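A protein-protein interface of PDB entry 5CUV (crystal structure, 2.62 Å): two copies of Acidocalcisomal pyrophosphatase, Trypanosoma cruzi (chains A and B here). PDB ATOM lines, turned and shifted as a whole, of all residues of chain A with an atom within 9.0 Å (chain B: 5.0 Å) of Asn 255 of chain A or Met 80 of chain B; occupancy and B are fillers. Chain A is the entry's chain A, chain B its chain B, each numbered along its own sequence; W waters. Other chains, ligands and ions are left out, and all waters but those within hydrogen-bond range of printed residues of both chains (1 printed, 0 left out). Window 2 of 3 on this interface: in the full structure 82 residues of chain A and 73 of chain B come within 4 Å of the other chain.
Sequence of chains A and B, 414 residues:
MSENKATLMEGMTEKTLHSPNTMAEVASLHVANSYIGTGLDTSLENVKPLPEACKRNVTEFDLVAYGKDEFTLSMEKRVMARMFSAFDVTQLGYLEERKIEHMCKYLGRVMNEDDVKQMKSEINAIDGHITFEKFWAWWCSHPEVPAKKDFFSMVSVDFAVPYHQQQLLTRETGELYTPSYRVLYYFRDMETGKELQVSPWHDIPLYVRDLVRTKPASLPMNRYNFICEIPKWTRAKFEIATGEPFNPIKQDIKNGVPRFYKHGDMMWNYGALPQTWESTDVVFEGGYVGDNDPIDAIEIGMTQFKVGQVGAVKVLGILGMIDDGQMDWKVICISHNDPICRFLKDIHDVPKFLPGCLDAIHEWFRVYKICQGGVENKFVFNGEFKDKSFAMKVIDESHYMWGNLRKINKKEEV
ND2 of Asn 255 of chain A lies within hydrogen-bond range of OE2 of Glu 76 of chain B (3.1 Å). OD1 of Asn 255 of chain A is in hydrogen-bond range of NE1 of Trp 139 of chain B (2.8 Å). The side-chain sulfur (SD) of Met 80 of chain B sits close to the backbone carbonyl oxygen (O) of Asn 255 of chain A.
The indole nitrogen (NE1) of Trp 139 of chain B lies close to the side-chain sulfur (SD) of Met 80 of chain B (3.5 Å).
Glu 76 of chain B touches Lys 254 of chain A (OE2 to O, 3.7 Å). Gly 256 of chain A touches Val 79 of chain B (O to CG1, 3.4 Å). Val 257 of chain A touches Glu 76 of chain B.
Asn 255 of chain A touches just these residues of chain B: Glu 76, Met 80 and Trp 139. Printed residues of chain A within 4 Å of Met 80 of chain B: Asn 255 (3.1 Å). Of chain A, only Gly 256 (3.4 Å) comes within 4 Å of Val 79 of chain B. Printed residues of chain A within 4 Å of Glu 76 of chain B: Lys 254 (3.7 Å), Asn 255 (3.1 Å) and Val 257 (3.5 Å). Of the printed residues of chain B, Val 257 of chain A touches Glu 76 (3.5 Å). Printed residues of chain A within 4 Å of Trp 139 of chain B: Asn 255 (2.8 Å). Printed residues of chain B within 4 Å of Gly 256 of chain A: Val 79 (3.4 Å). The nearest residue of chain B that does not touch Asn 255 of chain A is Leu 107 of chain B (4.7 Å). The nearest residue of chain A that does not touch Met 80 of chain B is Gly 256 of chain A (4.5 Å). The nearest printed residue of chain B that does not touch Lys 254 of chain A is Leu 107 of chain B (5.8 Å).
Of the 9 printed residues of chain A, 4 touch a printed residue of chain B. Hydrophobic or aromatic side chains of chain A that line the printed part of chain B: Val 257. Hydrophobic or aromatic side chains of chain B that line the printed part of chain A: Val 79, Met 80 and Trp 139. Among the printed residues, 6 pairs touch across the chains. Among the printed residues, no Asp or Glu carboxylate lies within 4 Å of a Lys or Arg side-chain nitrogen of the other chain.
No position is printed for both chains. Of the 6 pairs that touch across the chains among the printed residues, none has its exchanged pair printed and touching as well.
Water W1 lies within hydrogen-bond range of O of Leu 107 of chain B, N of Gly 256 of chain A, O of Ile 253 of chain A and N of Asn 255 of chain A.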
ATOM      1  N   PRO A 179     -17.249  -9.725   4.307  1.00  0.00           N
ATOM      2  CA  PRO A 179     -18.687 -10.061   4.326  1.00  0.00           C
ATOM      3  C   PRO A 179     -19.067 -11.507   3.986  1.00  0.00           C
ATOM      4  O   PRO A 179     -20.231 -11.872   4.061  1.00  0.00           O
ATOM      5  CB  PRO A 179     -19.296  -9.095   3.321  1.00  0.00           C
ATOM      6  CG  PRO A 179     -18.258  -8.020   3.102  1.00  0.00           C
ATOM      7  CD  PRO A 179     -16.959  -8.787   3.211  1.00  0.00           C
ATOM      8  N   ASP A 252     -20.197  -8.411  11.721  1.00  0.00           N
ATOM      9  CA  ASP A 252     -20.865  -7.149  11.511  1.00  0.00           C
ATOM     10  C   ASP A 252     -19.921  -6.281  10.718  1.00  0.00           C
ATOM     11  O   ASP A 252     -18.929  -5.754  11.250  1.00  0.00           O
ATOM     12  CB  ASP A 252     -21.194  -6.468  12.820  1.00  0.00           C
ATOM     13  CG  ASP A 252     -22.034  -5.214  12.619  1.00  0.00           C
ATOM     14  OD1 ASP A 252     -22.592  -5.026  11.508  1.00  0.00           O
ATOM     15  OD2 ASP A 252     -22.145  -4.420  13.579  1.00  0.00           O
ATOM     16  N   ILE A 253     -20.231  -6.176   9.427  1.00  0.00           N
ATOM     17  CA  ILE A 253     -19.458  -5.388   8.494  1.00  0.00           C
ATOM     18  C   ILE A 253     -20.374  -4.312   7.966  1.00  0.00           C
ATOM     19  O   ILE A 253     -21.509  -4.584   7.584  1.00  0.00           O
ATOM     20  CB  ILE A 253     -19.013  -6.224   7.300  1.00  0.00           C
ATOM     21  CG1 ILE A 253     -18.518  -7.600   7.748  1.00  0.00           C
ATOM     22  CG2 ILE A 253     -17.947  -5.482   6.559  1.00  0.00           C
ATOM     23  CD1 ILE A 253     -17.311  -7.546   8.698  1.00  0.00           C
ATOM     24  N   LYS A 254     -19.893  -3.083   7.973  1.00  0.00           N
ATOM     25  CA  LYS A 254     -20.651  -1.959   7.459  1.00  0.00           C
ATOM     26  C   LYS A 254     -19.684  -1.285   6.462  1.00  0.00           C
ATOM     27  O   LYS A 254     -18.479  -1.140   6.730  1.00  0.00           O
ATOM     28  CB  LYS A 254     -21.048  -1.022   8.594  1.00  0.00           C
ATOM     29  CG  LYS A 254     -22.222  -0.150   8.259  1.00  0.00           C
ATOM     30  CD  LYS A 254     -22.381   0.901   9.346  1.00  0.00           C
ATOM     31  CE  LYS A 254     -23.549   1.900   9.068  1.00  0.00           C
ATOM     32  NZ  LYS A 254     -23.629   2.955  10.147  1.00  0.00           N
ATOM     33  N   ASN A 255     -20.206  -0.922   5.295  1.00  0.00           N
ATOM     34  CA  ASN A 255     -19.376  -0.321   4.244  1.00  0.00           C
ATOM     35  C   ASN A 255     -18.039  -1.110   3.997  1.00  0.00           C
ATOM     36  O   ASN A 255     -16.994  -0.528   3.691  1.00  0.00           O
ATOM     37  CB  ASN A 255     -19.134   1.163   4.550  1.00  0.00           C
ATOM     38  CG  ASN A 255     -20.444   1.891   4.954  1.00  0.00           C
ATOM     39  OD1 ASN A 255     -21.447   1.874   4.212  1.00  0.00           O
ATOM     40  ND2 ASN A 255     -20.442   2.515   6.132  1.00  0.00           N
ATOM     41  N   GLY A 256     -18.117  -2.443   4.116  1.00  0.00           N
ATOM     42  CA  GLY A 256     -16.961  -3.278   3.880  1.00  0.00           C
ATOM     43  C   GLY A 256     -15.905  -3.290   4.985  1.00  0.00           C
ATOM     44  O   GLY A 256     -14.855  -3.923   4.883  1.00  0.00           O
ATOM     45  N   VAL A 257     -16.172  -2.599   6.074  1.00  0.00           N
ATOM     46  CA  VAL A 257     -15.207  -2.560   7.157  1.00  0.00           C
ATOM     47  C   VAL A 257     -15.844  -3.225   8.369  1.00  0.00           C
ATOM     48  O   VAL A 257     -16.891  -2.813   8.855  1.00  0.00           O
ATOM     49  CB  VAL A 257     -14.858  -1.118   7.419  1.00  0.00           C
ATOM     50  CG1 VAL A 257     -13.812  -0.983   8.498  1.00  0.00           C
ATOM     51  CG2 VAL A 257     -14.400  -0.532   6.148  1.00  0.00           C
ATOM     52  N   PRO A 258     -15.247  -4.300   8.838  1.00  0.00           N
ATOM     53  CA  PRO A 258     -15.804  -4.997  10.018  1.00  0.00           C
ATOM     54  C   PRO A 258     -15.968  -4.061  11.189  1.00  0.00           C
ATOM     55  O   PRO A 258     -15.168  -3.172  11.349  1.00  0.00           O
ATOM     56  CB  PRO A 258     -14.751  -6.085  10.328  1.00  0.00           C
ATOM     57  CG  PRO A 258     -13.474  -5.475   9.815  1.00  0.00           C
ATOM     58  CD  PRO A 258     -13.931  -4.843   8.473  1.00  0.00           C
ATOM     59  N   ARG A 259     -16.990  -4.282  12.008  1.00  0.00           N
ATOM     60  CA  ARG A 259     -17.257  -3.462  13.210  1.00  0.00           C
ATOM     61  C   ARG A 259     -16.678  -4.031  14.482  1.00  0.00           C
ATOM     62  O   ARG A 259     -16.527  -5.240  14.616  1.00  0.00           O
ATOM     63  CB  ARG A 259     -18.752  -3.279  13.428  1.00  0.00           C
ATOM     64  CG  ARG A 259     -19.376  -2.336  12.470  1.00  0.00           C
ATOM     65  CD  ARG A 259     -18.761  -1.019  12.705  1.00  0.00           C
ATOM     66  NE  ARG A 259     -19.503  -0.002  11.989  1.00  0.00           N
ATOM     67  CZ  ARG A 259     -19.429   1.306  12.218  1.00  0.00           C
ATOM     68  NH1 ARG A 259     -20.176   2.111  11.459  1.00  0.00           N
ATOM     69  NH2 ARG A 259     -18.638   1.814  13.186  1.00  0.00           N
ATOM     70  N   GLU B  76     -12.989   3.164   4.967  1.00  0.00           N
ATOM     71  CA  GLU B  76     -14.139   2.539   4.311  1.00  0.00           C
ATOM     72  C   GLU B  76     -13.999   2.834   2.798  1.00  0.00           C
ATOM     73  O   GLU B  76     -14.218   1.948   1.965  1.00  0.00           O
ATOM     74  CB  GLU B  76     -15.511   3.011   4.848  1.00  0.00           C
ATOM     75  CG  GLU B  76     -15.728   2.710   6.348  1.00  0.00           C
ATOM     76  CD  GLU B  76     -17.112   3.132   6.893  1.00  0.00           C
ATOM     77  OE1 GLU B  76     -17.552   4.269   6.593  1.00  0.00           O
ATOM     78  OE2 GLU B  76     -17.733   2.323   7.640  1.00  0.00           O
ATOM     79  N   LYS B  77     -13.618   4.066   2.449  1.00  0.00           N
ATOM     80  CA  LYS B  77     -13.445   4.432   1.043  1.00  0.00           C
ATOM     81  C   LYS B  77     -12.374   3.548   0.450  1.00  0.00           C
ATOM     82  O   LYS B  77     -12.566   2.939  -0.591  1.00  0.00           O
ATOM     83  CB  LYS B  77     -13.004   5.885   0.877  1.00  0.00           C
ATOM     84  CG  LYS B  77     -13.322   6.480  -0.494  1.00  0.00           C
ATOM     85  CD  LYS B  77     -12.334   7.597  -0.859  1.00  0.00           C
ATOM     86  CE  LYS B  77     -12.960   8.781  -1.606  1.00  0.00           C
ATOM     87  NZ  LYS B  77     -13.481   9.814  -0.653  1.00  0.00           N
ATOM     88  N   ARG B  78     -11.237   3.458   1.113  1.00  0.00           N
ATOM     89  CA  ARG B  78     -10.182   2.634   0.561  1.00  0.00           C
ATOM     90  C   ARG B  78     -10.494   1.167   0.420  1.00  0.00           C
ATOM     91  O   ARG B  78      -9.973   0.518  -0.485  1.00  0.00           O
ATOM     92  CB  ARG B  78      -8.902   2.780   1.358  1.00  0.00           C
ATOM     93  CG  ARG B  78      -8.050   3.959   0.961  1.00  0.00           C
ATOM     94  CD  ARG B  78      -8.112   4.278  -0.573  1.00  0.00           C
ATOM     95  NE  ARG B  78      -8.899   5.489  -0.847  1.00  0.00           N
ATOM     96  CZ  ARG B  78      -8.896   6.585  -0.073  1.00  0.00           C
ATOM     97  NH1 ARG B  78      -8.154   6.638   1.039  1.00  0.00           N
ATOM     98  NH2 ARG B  78      -9.631   7.642  -0.417  1.00  0.00           N
ATOM     99  N   VAL B  79     -11.319   0.626   1.317  1.00  0.00           N
ATOM    100  CA  VAL B  79     -11.670  -0.795   1.240  1.00  0.00           C
ATOM    101  C   VAL B  79     -12.698  -1.071   0.172  1.00  0.00           C
ATOM    102  O   VAL B  79     -12.577  -2.052  -0.552  1.00  0.00           O
ATOM    103  CB  VAL B  79     -12.192  -1.374   2.595  1.00  0.00           C
ATOM    104  CG1 VAL B  79     -12.773  -2.801   2.388  1.00  0.00           C
ATOM    105  CG2 VAL B  79     -11.062  -1.425   3.594  1.00  0.00           C
ATOM    106  N   MET B  80     -13.709  -0.209   0.076  1.00  0.00           N
ATOM    107  CA  MET B  80     -14.754  -0.388  -0.935  1.00  0.00           C
ATOM    108  C   MET B  80     -14.275  -0.025  -2.331  1.00  0.00           C
ATOM    109  O   MET B  80     -14.926  -0.337  -3.318  1.00  0.00           O
ATOM    110  CB  MET B  80     -15.944   0.512  -0.605  1.00  0.00           C
ATOM    111  CG  MET B  80     -16.694   0.096   0.650  1.00  0.00           C
ATOM    112  SD  MET B  80     -18.136   1.263   1.136  1.00  0.00           S
ATOM    113  CE  MET B  80     -19.379   0.776  -0.285  1.00  0.00           C
ATOM    114  N   ALA B  81     -13.106   0.605  -2.385  1.00  0.00           N
ATOM    115  CA  ALA B  81     -12.474   1.000  -3.627  1.00  0.00           C
ATOM    116  C   ALA B  81     -11.913  -0.296  -4.161  1.00  0.00           C
ATOM    117  O   ALA B  81     -12.335  -0.775  -5.209  1.00  0.00           O
ATOM    118  CB  ALA B  81     -11.357   1.991  -3.402  1.00  0.00           C
ATOM    119  N   ARG B  82     -10.972  -0.870  -3.420  1.00  0.00           N
ATOM    120  CA  ARG B  82     -10.314  -2.115  -3.797  1.00  0.00           C
ATOM    121  C   ARG B  82     -11.351  -3.167  -4.107  1.00  0.00           C
ATOM    122  O   ARG B  82     -11.168  -4.002  -4.997  1.00  0.00           O
ATOM    123  CB  ARG B  82      -9.392  -2.575  -2.673  1.00  0.00           C
ATOM    124  CG  ARG B  82      -8.332  -1.525  -2.308  1.00  0.00           C
ATOM    125  CD  ARG B  82      -7.063  -2.186  -1.790  1.00  0.00           C
ATOM    126  NE  ARG B  82      -7.355  -2.928  -0.566  1.00  0.00           N
ATOM    127  CZ  ARG B  82      -7.243  -2.436   0.667  1.00  0.00           C
ATOM    128  NH1 ARG B  82      -6.829  -1.182   0.859  1.00  0.00           N
ATOM    129  NH2 ARG B  82      -7.564  -3.202   1.702  1.00  0.00           N
ATOM    130  N   MET B  83     -12.455  -3.125  -3.383  1.00  0.00           N
ATOM    131  CA  MET B  83     -13.518  -4.065  -3.636  1.00  0.00           C
ATOM    132  C   MET B  83     -14.096  -3.757  -5.009  1.00  0.00           C
ATOM    133  O   MET B  83     -14.383  -4.672  -5.782  1.00  0.00           O
ATOM    134  CB  MET B  83     -14.589  -3.966  -2.551  1.00  0.00           C
ATOM    135  CG  MET B  83     -15.706  -4.984  -2.703  1.00  0.00           C
ATOM    136  SD  MET B  83     -17.000  -4.960  -1.288  1.00  0.00           S
ATOM    137  CE  MET B  83     -15.964  -5.923   0.054  1.00  0.00           C
ATOM    138  N   PHE B  84     -14.266  -2.473  -5.320  1.00  0.00           N
ATOM    139  CA  PHE B  84     -14.794  -2.058  -6.635  1.00  0.00           C
ATOM    140  C   PHE B  84     -13.865  -2.528  -7.751  1.00  0.00           C
ATOM    141  O   PHE B  84     -14.308  -3.043  -8.765  1.00  0.00           O
ATOM    142  CB  PHE B  84     -14.901  -0.528  -6.678  1.00  0.00           C
ATOM    143  CG  PHE B  84     -15.505   0.020  -7.940  1.00  0.00           C
ATOM    144  CD1 PHE B  84     -14.706   0.246  -9.070  1.00  0.00           C
ATOM    145  CD2 PHE B  84     -16.864   0.362  -7.987  1.00  0.00           C
ATOM    146  CE1 PHE B  84     -15.255   0.817 -10.242  1.00  0.00           C
ATOM    147  CE2 PHE B  84     -17.425   0.928  -9.131  1.00  0.00           C
ATOM    148  CZ  PHE B  84     -16.619   1.159 -10.266  1.00  0.00           C
ATOM    149  N   MET B 103     -22.519  -6.066  -5.958  1.00  0.00           N
ATOM    150  CA  MET B 103     -21.758  -5.556  -4.911  1.00  0.00           C
ATOM    151  C   MET B 103     -22.555  -4.983  -3.807  1.00  0.00           C
ATOM    152  O   MET B 103     -22.530  -5.226  -2.698  1.00  0.00           O
ATOM    153  CB  MET B 103     -20.922  -4.572  -5.609  1.00  0.00           C
ATOM    154  CG  MET B 103     -19.845  -4.140  -4.732  1.00  0.00           C
ATOM    155  SD  MET B 103     -18.596  -3.023  -5.543  1.00  0.00           S
ATOM    156  CE  MET B 103     -17.952  -1.617  -4.587  1.00  0.00           C
ATOM    157  N   LEU B 107     -22.030  -5.977  -0.125  1.00  0.00           N
ATOM    158  CA  LEU B 107     -21.733  -5.081   0.964  1.00  0.00           C
ATOM    159  C   LEU B 107     -22.938  -5.079   1.881  1.00  0.00           C
ATOM    160  O   LEU B 107     -23.081  -4.205   2.743  1.00  0.00           O
ATOM    161  CB  LEU B 107     -21.455  -3.689   0.450  1.00  0.00           C
ATOM    162  CG  LEU B 107     -20.201  -3.705  -0.412  1.00  0.00           C
ATOM    163  CD1 LEU B 107     -19.918  -2.329  -1.048  1.00  0.00           C
ATOM    164  CD2 LEU B 107     -19.060  -4.146   0.494  1.00  0.00           C
ATOM    165  N   PHE B 132     -16.116   4.760  -9.827  1.00  0.00           N
ATOM    166  CA  PHE B 132     -16.182   4.570  -8.392  1.00  0.00           C
ATOM    167  C   PHE B 132     -16.652   5.857  -7.712  1.00  0.00           C
ATOM    168  O   PHE B 132     -17.492   5.818  -6.820  1.00  0.00           O
ATOM    169  CB  PHE B 132     -14.812   4.173  -7.853  1.00  0.00           C
ATOM    170  CG  PHE B 132     -14.788   3.961  -6.379  1.00  0.00           C
ATOM    171  CD1 PHE B 132     -15.771   3.206  -5.764  1.00  0.00           C
ATOM    172  CD2 PHE B 132     -13.756   4.468  -5.614  1.00  0.00           C
ATOM    173  CE1 PHE B 132     -15.721   2.955  -4.421  1.00  0.00           C
ATOM    174  CE2 PHE B 132     -13.701   4.221  -4.269  1.00  0.00           C
ATOM    175  CZ  PHE B 132     -14.683   3.462  -3.671  1.00  0.00           C
ATOM    176  N   PHE B 135     -20.109   6.080  -7.884  1.00  0.00           N
ATOM    177  CA  PHE B 135     -20.643   5.089  -6.969  1.00  0.00           C
ATOM    178  C   PHE B 135     -20.513   5.531  -5.513  1.00  0.00           C
ATOM    179  O   PHE B 135     -21.503   5.610  -4.800  1.00  0.00           O
ATOM    180  CB  PHE B 135     -19.932   3.754  -7.180  1.00  0.00           C
ATOM    181  CG  PHE B 135     -20.472   2.676  -6.337  1.00  0.00           C
ATOM    182  CD1 PHE B 135     -21.763   2.207  -6.546  1.00  0.00           C
ATOM    183  CD2 PHE B 135     -19.755   2.211  -5.246  1.00  0.00           C
ATOM    184  CE1 PHE B 135     -22.340   1.299  -5.670  1.00  0.00           C
ATOM    185  CE2 PHE B 135     -20.318   1.304  -4.361  1.00  0.00           C
ATOM    186  CZ  PHE B 135     -21.609   0.848  -4.568  1.00  0.00           C
ATOM    187  N   TRP B 136     -19.278   5.813  -5.100  1.00  0.00           N
ATOM    188  CA  TRP B 136     -18.970   6.250  -3.736  1.00  0.00           C
ATOM    189  C   TRP B 136     -19.817   7.424  -3.277  1.00  0.00           C
ATOM    190  O   TRP B 136     -20.379   7.401  -2.177  1.00  0.00           O
ATOM    191  CB  TRP B 136     -17.503   6.660  -3.607  1.00  0.00           C
ATOM    192  CG  TRP B 136     -17.105   7.039  -2.204  1.00  0.00           C
ATOM    193  CD1 TRP B 136     -16.587   8.224  -1.805  1.00  0.00           C
ATOM    194  CD2 TRP B 136     -17.094   6.179  -1.033  1.00  0.00           C
ATOM    195  NE1 TRP B 136     -16.238   8.169  -0.470  1.00  0.00           N
ATOM    196  CE2 TRP B 136     -16.537   6.929   0.027  1.00  0.00           C
ATOM    197  CE3 TRP B 136     -17.493   4.845  -0.788  1.00  0.00           C
ATOM    198  CZ2 TRP B 136     -16.361   6.401   1.307  1.00  0.00           C
ATOM    199  CZ3 TRP B 136     -17.320   4.315   0.479  1.00  0.00           C
ATOM    200  CH2 TRP B 136     -16.754   5.097   1.515  1.00  0.00           C
ATOM    201  N   TRP B 139     -23.033   6.149  -2.756  1.00  0.00           N
ATOM    202  CA  TRP B 139     -23.076   5.222  -1.646  1.00  0.00           C
ATOM    203  C   TRP B 139     -23.127   6.076  -0.401  1.00  0.00           C
ATOM    204  O   TRP B 139     -23.969   5.871   0.485  1.00  0.00           O
ATOM    205  CB  TRP B 139     -21.832   4.330  -1.648  1.00  0.00           C
ATOM    206  CG  TRP B 139     -21.792   3.400  -0.513  1.00  0.00           C
ATOM    207  CD1 TRP B 139     -21.140   3.578   0.639  1.00  0.00           C
ATOM    208  CD2 TRP B 139     -22.500   2.160  -0.396  1.00  0.00           C
ATOM    209  NE1 TRP B 139     -21.387   2.533   1.492  1.00  0.00           N
ATOM    210  CE2 TRP B 139     -22.220   1.645   0.877  1.00  0.00           C
ATOM    211  CE3 TRP B 139     -23.342   1.435  -1.247  1.00  0.00           C
ATOM    212  CZ2 TRP B 139     -22.749   0.437   1.331  1.00  0.00           C
ATOM    213  CZ3 TRP B 139     -23.868   0.231  -0.795  1.00  0.00           C
ATOM    214  CH2 TRP B 139     -23.568  -0.254   0.485  1.00  0.00           C
HETATM  215  O   HOH W   1     -20.767  -4.116   4.406  1.00  0.00           O
